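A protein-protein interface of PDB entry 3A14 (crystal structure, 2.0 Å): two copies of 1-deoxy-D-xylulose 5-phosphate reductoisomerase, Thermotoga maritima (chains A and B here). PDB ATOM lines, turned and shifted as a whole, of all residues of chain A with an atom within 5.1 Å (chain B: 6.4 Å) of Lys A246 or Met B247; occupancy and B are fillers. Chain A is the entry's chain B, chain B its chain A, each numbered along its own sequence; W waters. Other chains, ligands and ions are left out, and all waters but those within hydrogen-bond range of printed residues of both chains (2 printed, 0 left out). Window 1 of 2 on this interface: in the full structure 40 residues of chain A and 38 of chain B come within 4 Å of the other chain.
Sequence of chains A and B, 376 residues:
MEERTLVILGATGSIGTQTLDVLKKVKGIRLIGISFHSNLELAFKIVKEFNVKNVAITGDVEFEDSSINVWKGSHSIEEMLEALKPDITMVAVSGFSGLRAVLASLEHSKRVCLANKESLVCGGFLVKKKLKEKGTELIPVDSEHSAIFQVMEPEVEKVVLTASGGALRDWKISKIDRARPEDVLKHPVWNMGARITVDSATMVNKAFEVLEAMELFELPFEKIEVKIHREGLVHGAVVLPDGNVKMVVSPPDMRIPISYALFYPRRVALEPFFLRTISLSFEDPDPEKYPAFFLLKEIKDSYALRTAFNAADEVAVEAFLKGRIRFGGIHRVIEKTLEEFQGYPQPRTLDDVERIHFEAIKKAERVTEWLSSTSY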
ATOM      1  N   VAL A 151     -22.508  21.344   7.788  1.00  0.00           N
ATOM      2  CA  VAL A 151     -21.304  21.949   7.194  1.00  0.00           C
ATOM      3  C   VAL A 151     -21.409  22.079   5.654  1.00  0.00           C
ATOM      4  O   VAL A 151     -20.517  22.609   4.992  1.00  0.00           O
ATOM      5  CB  VAL A 151     -19.997  21.206   7.630  1.00  0.00           C
ATOM      6  CG1 VAL A 151     -19.669  21.422   9.134  1.00  0.00           C
ATOM      7  CG2 VAL A 151     -20.055  19.692   7.322  1.00  0.00           C
ATOM      8  N   MET A 152     -22.512  21.608   5.076  1.00  0.00           N
ATOM      9  CA  MET A 152     -22.654  21.606   3.623  1.00  0.00           C
ATOM     10  C   MET A 152     -22.560  23.023   3.027  1.00  0.00           C
ATOM     11  O   MET A 152     -23.044  23.989   3.605  1.00  0.00           O
ATOM     12  CB  MET A 152     -23.992  20.938   3.229  1.00  0.00           C
ATOM     13  CG  MET A 152     -24.249  20.780   1.745  1.00  0.00           C
ATOM     14  SD  MET A 152     -22.948  19.857   0.920  1.00  0.00           S
ATOM     15  CE  MET A 152     -23.449  20.140  -0.785  1.00  0.00           C
ATOM     16  N   GLU A 153     -21.930  23.147   1.869  1.00  0.00           N
ATOM     17  CA  GLU A 153     -22.052  24.382   1.101  1.00  0.00           C
ATOM     18  C   GLU A 153     -22.001  24.016  -0.375  1.00  0.00           C
ATOM     19  O   GLU A 153     -21.557  22.919  -0.702  1.00  0.00           O
ATOM     20  CB  GLU A 153     -20.962  25.405   1.501  1.00  0.00           C
ATOM     21  CG  GLU A 153     -19.582  24.856   1.527  1.00  0.00           C
ATOM     22  CD  GLU A 153     -18.544  25.897   1.926  1.00  0.00           C
ATOM     23  OE1 GLU A 153     -18.179  25.950   3.117  1.00  0.00           O
ATOM     24  OE2 GLU A 153     -18.104  26.665   1.051  1.00  0.00           O
ATOM     25  N   GLY A 236     -19.029  13.066   9.731  1.00  0.00           N
ATOM     26  CA  GLY A 236     -19.165  13.614   8.388  1.00  0.00           C
ATOM     27  C   GLY A 236     -18.129  14.681   8.188  1.00  0.00           C
ATOM     28  O   GLY A 236     -17.694  15.303   9.163  1.00  0.00           O
ATOM     29  N   ALA A 237     -17.750  14.901   6.931  1.00  0.00           N
ATOM     30  CA  ALA A 237     -16.793  15.955   6.580  1.00  0.00           C
ATOM     31  C   ALA A 237     -17.074  16.464   5.187  1.00  0.00           C
ATOM     32  O   ALA A 237     -17.643  15.746   4.344  1.00  0.00           O
ATOM     33  CB  ALA A 237     -15.331  15.438   6.671  1.00  0.00           C
ATOM     34  N   VAL A 238     -16.691  17.705   4.925  1.00  0.00           N
ATOM     35  CA  VAL A 238     -16.719  18.195   3.572  1.00  0.00           C
ATOM     36  C   VAL A 238     -15.338  18.735   3.260  1.00  0.00           C
ATOM     37  O   VAL A 238     -14.726  19.473   4.082  1.00  0.00           O
ATOM     38  CB  VAL A 238     -17.887  19.242   3.295  1.00  0.00           C
ATOM     39  CG1 VAL A 238     -19.275  18.626   3.629  1.00  0.00           C
ATOM     40  CG2 VAL A 238     -17.683  20.498   4.102  1.00  0.00           C
ATOM     41  N   LEU A 240     -13.206  21.052   0.777  1.00  0.00           N
ATOM     42  CA  LEU A 240     -13.463  22.259  -0.005  1.00  0.00           C
ATOM     43  C   LEU A 240     -12.370  22.368  -1.066  1.00  0.00           C
ATOM     44  O   LEU A 240     -11.274  21.841  -0.875  1.00  0.00           O
ATOM     45  CB  LEU A 240     -13.478  23.526   0.908  1.00  0.00           C
ATOM     46  CG  LEU A 240     -14.651  23.773   1.885  1.00  0.00           C
ATOM     47  CD1 LEU A 240     -16.031  23.416   1.218  1.00  0.00           C
ATOM     48  CD2 LEU A 240     -14.465  23.044   3.238  1.00  0.00           C
ATOM     49  N   ASN A 244      -9.389  23.681   2.771  1.00  0.00           N
ATOM     50  CA  ASN A 244     -10.083  23.610   4.048  1.00  0.00           C
ATOM     51  C   ASN A 244     -10.894  22.325   4.057  1.00  0.00           C
ATOM     52  O   ASN A 244     -11.358  21.844   3.013  1.00  0.00           O
ATOM     53  CB  ASN A 244     -11.055  24.796   4.212  1.00  0.00           C
ATOM     54  CG  ASN A 244     -10.357  26.087   4.631  1.00  0.00           C
ATOM     55  OD1 ASN A 244     -10.380  27.108   3.916  1.00  0.00           O
ATOM     56  ND2 ASN A 244      -9.730  26.045   5.783  1.00  0.00           N
ATOM     57  N   VAL A 245     -11.064  21.769   5.239  1.00  0.00           N
ATOM     58  CA  VAL A 245     -11.964  20.635   5.410  1.00  0.00           C
ATOM     59  C   VAL A 245     -12.742  20.918   6.671  1.00  0.00           C
ATOM     60  O   VAL A 245     -12.143  21.247   7.732  1.00  0.00           O
ATOM     61  CB  VAL A 245     -11.172  19.278   5.602  1.00  0.00           C
ATOM     62  CG1 VAL A 245     -12.149  18.103   5.885  1.00  0.00           C
ATOM     63  CG2 VAL A 245     -10.330  18.978   4.397  1.00  0.00           C
ATOM     64  N   LYS A 246     -14.065  20.808   6.581  1.00  0.00           N
ATOM     65  CA  LYS A 246     -14.916  20.994   7.752  1.00  0.00           C
ATOM     66  C   LYS A 246     -15.389  19.639   8.225  1.00  0.00           C
ATOM     67  O   LYS A 246     -15.969  18.875   7.429  1.00  0.00           O
ATOM     68  CB  LYS A 246     -16.131  21.877   7.426  1.00  0.00           C
ATOM     69  CG  LYS A 246     -15.763  23.321   7.070  1.00  0.00           C
ATOM     70  CD  LYS A 246     -16.982  24.245   6.944  1.00  0.00           C
ATOM     71  CE  LYS A 246     -17.731  23.995   5.641  1.00  0.00           C
ATOM     72  NZ  LYS A 246     -18.924  24.896   5.516  1.00  0.00           N
ATOM     73  N   MET A 247     -15.114  19.335   9.490  1.00  0.00           N
ATOM     74  CA  MET A 247     -15.439  18.018  10.071  1.00  0.00           C
ATOM     75  C   MET A 247     -16.384  18.170  11.230  1.00  0.00           C
ATOM     76  O   MET A 247     -16.265  19.125  12.007  1.00  0.00           O
ATOM     77  CB  MET A 247     -14.191  17.309  10.604  1.00  0.00           C
ATOM     78  CG  MET A 247     -13.113  17.007   9.609  1.00  0.00           C
ATOM     79  SD  MET A 247     -11.873  15.838  10.251  1.00  0.00           S
ATOM     80  CE  MET A 247     -11.843  16.290  11.984  1.00  0.00           C
ATOM     81  N   VAL A 248     -17.317  17.221  11.359  1.00  0.00           N
ATOM     82  CA  VAL A 248     -18.220  17.192  12.502  1.00  0.00           C
ATOM     83  C   VAL A 248     -17.915  15.979  13.379  1.00  0.00           C
ATOM     84  O   VAL A 248     -17.921  14.845  12.909  1.00  0.00           O
ATOM     85  CB  VAL A 248     -19.693  17.234  12.045  1.00  0.00           C
ATOM     86  CG1 VAL A 248     -20.645  17.183  13.239  1.00  0.00           C
ATOM     87  CG2 VAL A 248     -19.943  18.496  11.186  1.00  0.00           C
ATOM     88  N   VAL A 249     -17.596  16.249  14.647  1.00  0.00           N
ATOM     89  CA  VAL A 249     -17.287  15.222  15.637  1.00  0.00           C
ATOM     90  C   VAL A 249     -18.354  15.235  16.705  1.00  0.00           C
ATOM     91  O   VAL A 249     -18.858  16.303  17.072  1.00  0.00           O
ATOM     92  CB  VAL A 249     -15.896  15.475  16.256  1.00  0.00           C
ATOM     93  CG1 VAL A 249     -15.707  14.674  17.527  1.00  0.00           C
ATOM     94  CG2 VAL A 249     -14.812  15.143  15.234  1.00  0.00           C
ATOM     95  N   LEU A 275     -12.493  18.474  23.730  1.00  0.00           N
ATOM     96  CA  LEU A 275     -11.407  17.962  22.893  1.00  0.00           C
ATOM     97  C   LEU A 275     -10.258  17.356  23.692  1.00  0.00           C
ATOM     98  O   LEU A 275      -9.821  17.921  24.693  1.00  0.00           O
ATOM     99  CB  LEU A 275     -10.879  19.062  21.960  1.00  0.00           C
ATOM    100  CG  LEU A 275     -11.836  19.638  20.910  1.00  0.00           C
ATOM    101  CD1 LEU A 275     -11.158  20.755  20.136  1.00  0.00           C
ATOM    102  CD2 LEU A 275     -12.347  18.550  19.963  1.00  0.00           C
ATOM    103  N   ILE A 278      -6.602  12.701  19.999  1.00  0.00           N
ATOM    104  CA  ILE A 278      -7.280  11.637  19.251  1.00  0.00           C
ATOM    105  C   ILE A 278      -6.481  11.251  18.014  1.00  0.00           C
ATOM    106  O   ILE A 278      -5.752  12.073  17.443  1.00  0.00           O
ATOM    107  CB  ILE A 278      -8.727  12.045  18.811  1.00  0.00           C
ATOM    108  CG1 ILE A 278      -8.776  13.500  18.307  1.00  0.00           C
ATOM    109  CG2 ILE A 278      -9.731  11.813  19.949  1.00  0.00           C
ATOM    110  CD1 ILE A 278     -10.215  14.045  18.040  1.00  0.00           C
ATOM    111  N   GLN B 150     -15.724  30.168   9.617  1.00  0.00           N
ATOM    112  CA  GLN B 150     -16.354  29.181   8.737  1.00  0.00           C
ATOM    113  C   GLN B 150     -17.285  28.218   9.483  1.00  0.00           C
ATOM    114  O   GLN B 150     -18.157  27.605   8.866  1.00  0.00           O
ATOM    115  CB  GLN B 150     -15.262  28.383   8.056  1.00  0.00           C
ATOM    116  CG  GLN B 150     -14.514  29.168   7.024  1.00  0.00           C
ATOM    117  CD  GLN B 150     -13.379  28.366   6.441  1.00  0.00           C
ATOM    118  OE1 GLN B 150     -13.593  27.337   5.790  1.00  0.00           O
ATOM    119  NE2 GLN B 150     -12.156  28.841   6.653  1.00  0.00           N
ATOM    120  N   VAL B 151     -17.110  28.083  10.795  1.00  0.00           N
ATOM    121  CA  VAL B 151     -17.968  27.181  11.573  1.00  0.00           C
ATOM    122  C   VAL B 151     -18.770  27.827  12.711  1.00  0.00           C
ATOM    123  O   VAL B 151     -19.533  27.132  13.391  1.00  0.00           O
ATOM    124  CB  VAL B 151     -17.176  25.956  12.127  1.00  0.00           C
ATOM    125  CG1 VAL B 151     -16.794  24.990  10.985  1.00  0.00           C
ATOM    126  CG2 VAL B 151     -15.912  26.409  12.907  1.00  0.00           C
ATOM    127  N   VAL B 234      -5.493  21.188  12.730  1.00  0.00           N
ATOM    128  CA  VAL B 234      -6.735  21.805  13.171  1.00  0.00           C
ATOM    129  C   VAL B 234      -6.477  23.286  13.468  1.00  0.00           C
ATOM    130  O   VAL B 234      -5.657  23.618  14.346  1.00  0.00           O
ATOM    131  CB  VAL B 234      -7.293  21.101  14.427  1.00  0.00           C
ATOM    132  CG1 VAL B 234      -8.521  21.821  14.970  1.00  0.00           C
ATOM    133  CG2 VAL B 234      -7.614  19.633  14.138  1.00  0.00           C
ATOM    134  N   GLY B 236      -9.097  25.532  14.087  1.00  0.00           N
ATOM    135  CA  GLY B 236     -10.091  26.059  14.987  1.00  0.00           C
ATOM    136  C   GLY B 236     -11.198  25.055  15.115  1.00  0.00           C
ATOM    137  O   GLY B 236     -11.420  24.215  14.203  1.00  0.00           O
ATOM    138  N   ALA B 237     -11.892  25.136  16.239  1.00  0.00           N
ATOM    139  CA  ALA B 237     -13.035  24.258  16.494  1.00  0.00           C
ATOM    140  C   ALA B 237     -14.088  25.015  17.308  1.00  0.00           C
ATOM    141  O   ALA B 237     -13.786  25.962  18.073  1.00  0.00           O
ATOM    142  CB  ALA B 237     -12.603  22.982  17.218  1.00  0.00           C
ATOM    143  N   VAL B 238     -15.320  24.575  17.143  1.00  0.00           N
ATOM    144  CA  VAL B 238     -16.451  25.149  17.842  1.00  0.00           C
ATOM    145  C   VAL B 238     -17.147  23.976  18.517  1.00  0.00           C
ATOM    146  O   VAL B 238     -17.528  23.012  17.858  1.00  0.00           O
ATOM    147  CB  VAL B 238     -17.346  25.941  16.858  1.00  0.00           C
ATOM    148  CG1 VAL B 238     -18.687  26.217  17.433  1.00  0.00           C
ATOM    149  CG2 VAL B 238     -16.649  27.279  16.511  1.00  0.00           C
ATOM    150  N   VAL B 245     -19.154  18.834  17.522  1.00  0.00           N
ATOM    151  CA  VAL B 245     -17.970  19.696  17.398  1.00  0.00           C
ATOM    152  C   VAL B 245     -17.685  19.876  15.913  1.00  0.00           C
ATOM    153  O   VAL B 245     -17.560  18.895  15.169  1.00  0.00           O
ATOM    154  CB  VAL B 245     -16.708  19.118  18.138  1.00  0.00           C
ATOM    155  CG1 VAL B 245     -15.519  20.071  18.029  1.00  0.00           C
ATOM    156  CG2 VAL B 245     -17.035  18.854  19.606  1.00  0.00           C
ATOM    157  N   LYS B 246     -17.631  21.132  15.485  1.00  0.00           N
ATOM    158  CA  LYS B 246     -17.251  21.443  14.121  1.00  0.00           C
ATOM    159  C   LYS B 246     -15.803  21.901  14.125  1.00  0.00           C
ATOM    160  O   LYS B 246     -15.455  22.886  14.810  1.00  0.00           O
ATOM    161  CB  LYS B 246     -18.155  22.537  13.547  1.00  0.00           C
ATOM    162  CG  LYS B 246     -19.611  22.161  13.460  1.00  0.00           C
ATOM    163  CD  LYS B 246     -20.370  23.113  12.511  1.00  0.00           C
ATOM    164  CE  LYS B 246     -21.032  24.166  13.234  1.00  0.00           C
ATOM    165  NZ  LYS B 246     -21.331  25.282  12.274  1.00  0.00           N
ATOM    166  N   MET B 247     -14.969  21.198  13.373  1.00  0.00           N
ATOM    167  CA  MET B 247     -13.548  21.520  13.319  1.00  0.00           C
ATOM    168  C   MET B 247     -13.162  21.861  11.911  1.00  0.00           C
ATOM    169  O   MET B 247     -13.713  21.288  10.946  1.00  0.00           O
ATOM    170  CB  MET B 247     -12.685  20.324  13.704  1.00  0.00           C
ATOM    171  CG  MET B 247     -12.910  19.733  15.036  1.00  0.00           C
ATOM    172  SD  MET B 247     -11.600  18.499  15.275  1.00  0.00           S
ATOM    173  CE  MET B 247     -12.390  17.515  16.544  1.00  0.00           C
ATOM    174  N   VAL B 248     -12.165  22.722  11.793  1.00  0.00           N
ATOM    175  CA  VAL B 248     -11.599  23.065  10.498  1.00  0.00           C
ATOM    176  C   VAL B 248     -10.151  22.600  10.427  1.00  0.00           C
ATOM    177  O   VAL B 248      -9.328  22.947  11.289  1.00  0.00           O
ATOM    178  CB  VAL B 248     -11.738  24.568  10.166  1.00  0.00           C
ATOM    179  CG1 VAL B 248     -11.116  24.881   8.794  1.00  0.00           C
ATOM    180  CG2 VAL B 248     -13.224  24.961  10.162  1.00  0.00           C
ATOM    181  N   VAL B 249      -9.878  21.780   9.409  1.00  0.00           N
ATOM    182  CA  VAL B 249      -8.540  21.280   9.123  1.00  0.00           C
ATOM    183  C   VAL B 249      -8.071  21.844   7.792  1.00  0.00           C
ATOM    184  O   VAL B 249      -8.851  21.983   6.869  1.00  0.00           O
ATOM    185  CB  VAL B 249      -8.533  19.740   9.033  1.00  0.00           C
ATOM    186  CG1 VAL B 249      -7.188  19.245   8.580  1.00  0.00           C
ATOM    187  CG2 VAL B 249      -8.892  19.135  10.364  1.00  0.00           C
ATOM    188  N   ARG B 267     -15.539  29.578  -3.107  1.00  0.00           N
ATOM    189  CA  ARG B 267     -14.351  28.803  -2.703  1.00  0.00           C
ATOM    190  C   ARG B 267     -13.417  28.778  -3.903  1.00  0.00           C
ATOM    191  O   ARG B 267     -13.819  28.374  -4.986  1.00  0.00           O
ATOM    192  CB  ARG B 267     -14.727  27.366  -2.309  1.00  0.00           C
ATOM    193  CG  ARG B 267     -15.562  27.236  -1.042  1.00  0.00           C
ATOM    194  CD  ARG B 267     -14.691  27.431   0.243  1.00  0.00           C
ATOM    195  NE  ARG B 267     -15.450  27.244   1.487  1.00  0.00           N
ATOM    196  CZ  ARG B 267     -14.911  27.273   2.691  1.00  0.00           C
ATOM    197  NH1 ARG B 267     -13.605  27.457   2.800  1.00  0.00           N
ATOM    198  NH2 ARG B 267     -15.660  27.075   3.782  1.00  0.00           N
ATOM    199  N   LEU B 280      -4.010  13.921  16.184  1.00  0.00           N
ATOM    200  CA  LEU B 280      -4.517  15.208  16.661  1.00  0.00           C
ATOM    201  C   LEU B 280      -4.345  15.324  18.173  1.00  0.00           C
ATOM    202  O   LEU B 280      -5.179  14.847  18.940  1.00  0.00           O
ATOM    203  CB  LEU B 280      -5.988  15.431  16.248  1.00  0.00           C
ATOM    204  CG  LEU B 280      -6.411  15.484  14.766  1.00  0.00           C
ATOM    205  CD1 LEU B 280      -7.872  15.902  14.643  1.00  0.00           C
ATOM    206  CD2 LEU B 280      -5.554  16.412  13.920  1.00  0.00           C
ATOM    207  N   PHE B 282      -4.029  17.592  21.705  1.00  0.00           N
ATOM    208  CA  PHE B 282      -4.486  18.832  22.341  1.00  0.00           C
ATOM    209  C   PHE B 282      -4.108  18.888  23.832  1.00  0.00           C
ATOM    210  O   PHE B 282      -4.654  18.135  24.650  1.00  0.00           O
ATOM    211  CB  PHE B 282      -6.011  19.006  22.183  1.00  0.00           C
ATOM    212  CG  PHE B 282      -6.483  18.959  20.756  1.00  0.00           C
ATOM    213  CD1 PHE B 282      -6.370  20.071  19.930  1.00  0.00           C
ATOM    214  CD2 PHE B 282      -7.024  17.792  20.230  1.00  0.00           C
ATOM    215  CE1 PHE B 282      -6.793  20.014  18.599  1.00  0.00           C
ATOM    216  CE2 PHE B 282      -7.448  17.730  18.898  1.00  0.00           C
ATOM    217  CZ  PHE B 282      -7.335  18.844  18.090  1.00  0.00           C
HETATM  218  O   HOH W   1     -18.108  27.501   6.164  1.00  0.00           O
HETATM  219  O   HOH W   2      -9.302  29.371   5.676  1.00  0.00           O
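Of the 14 printed residues of chain B, 9 touch a printed residue of chain A. Hydrophobic or aromatic side chains of chain B within 4 Å of the printed part of chain A: Ala B237, Val B245, Met B247, Val B248 and Leu B280. Of the 15 printed residues of chain A, 11 touch a printed residue of chain B. Hydrophobic or aromatic side chains of chain A within 4 Å of the printed part of chain B: Val A151, Leu A240, Val A245, Met A247, Val A249, Leu A275 and Ile A278. Among the printed residues, 20 pairs touch across the chains. Among the printed residues, Asp or Glu carboxylates within 4 Å of a Lys or Arg side-chain nitrogen of the other chain: Glu A153 with Arg B267 (2.8 Å).
Lys A246 touches just one residue of chain B: Met B247. Of chain A, only Val A245 (3.6 Å), Lys A246 (3.4 Å), Met A247 (2.8 Å), Val A249 (3.6 Å) and Leu A275 (3.6 Å) come within 4 Å of Met B247. Printed residues of chain B within 4 Å of Val A249: Val B245 (2.6 Å) and Met B247 (3.6 Å). Printed residues of chain A within 4 Å of Gln B150: Asn A244 (3.7 Å). Printed residues of chain A within 4 Å of Val B245: Met A247, Val A248 and Val A249. Ala A237 touches none of the printed residues of chain B. The nearest residue of chain B that does not touch Lys A246 is Gln B150 (4.05 Å). The nearest residue of chain A that does not touch Met B247 is Ile A278 (4.4 Å).
Water W1 lies within hydrogen-bond range of O of Gln B150 (2.7 Å), NZ of Lys A246 (2.8 Å), OE1 of Glu A153 (3.4 Å) and NH2 of Arg B267 (3.4 Å). Water W2 lies within hydrogen-bond range of OD1 of Asn A244 (3.1 Å) and NE2 of Gln B150 (3.1 Å).
O of Met A247 sits at hydrogen-bond distance from N of Met B247 (2.8 Å). O of Val B245 sits close to O of Met A247 (3.4 Å). NH1 of Arg B267 sits at hydrogen-bond distance from OD1 of Asn A244 (3.4 Å). The backbone carbonyl oxygen of Leu B280 is in hydrogen-bond range of the backbone NH of Ile A278 (2.8 Å). The guanidinium group of Arg B267 lies within salt-bridge range of the side-chain carboxylate of Glu A153 (2.8 Å). O of Val A249 sits at hydrogen-bond distance from N of Val B245 (2.6 Å). The backbone NH (N) of Val A245 lies within hydrogen-bond range of the backbone carbonyl oxygen (O) of Val B249 (2.8 Å).
N of Val A238 lies within hydrogen-bond range of O of Lys A246 (2.9 Å). The backbone carbonyl oxygen (O) of Gly B236 is in hydrogen-bond range of the backbone NH (N) of Val B248 (2.9 Å). OE1 of Gln B150 lies within hydrogen-bond range of NH2 of Arg B267 (2.9 Å). The backbone carbonyl oxygen (O) of Gly A236 sits at hydrogen-bond distance from the backbone NH (N) of Val A248. The backbone carbonyl oxygen of Val A151 is in hydrogen-bond range of the side-chain amino group of Lys A246. The side-chain carboxylate (OE1) of Glu A153 lies within salt-bridge range of the side-chain amino group (NZ) of Lys A246 (2.7 Å).
Val A151 touches Lys B246, but with the chains exchanged Lys A246 does not touch Val B151 (4.1 Å). Val A245 touches Val B249, and with the chains exchanged Val A249 touches Val B245. Lys A246 touches Met B247, and with the chains exchanged Met A247 touches Lys B246. Val A249 touches Met B247, but with the chains exchanged Met A247 does not touch Val B249 (4.4 Å). Of the 20 pairs that touch across the chains among the printed residues, 9 have their exchanged pair printed and touching as well.
CD of Lys B246 touches CG1 of Val A151, 3.8 Å away. Leu A240 touches Arg B267 (CG to NE, 3.6 Å). Gln B150 touches Asn A244 (OE1 to CG, 3.7 Å). ND2 of Asn A244 touches CG1 of Val B248 (3.5 Å). Asn A244 touches Val B249. Val A245 touches Met B247. Met A247 touches Lys B246 (O to CA, 3.3 Å). Val A248 touches Val B245 (CA to O, 3.2 Å). CD1 of Leu A275 touches CB of Ala B237, 3.9 Å away. Leu A275 touches Met B247 (CD2 to CE, 3.6 Å).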
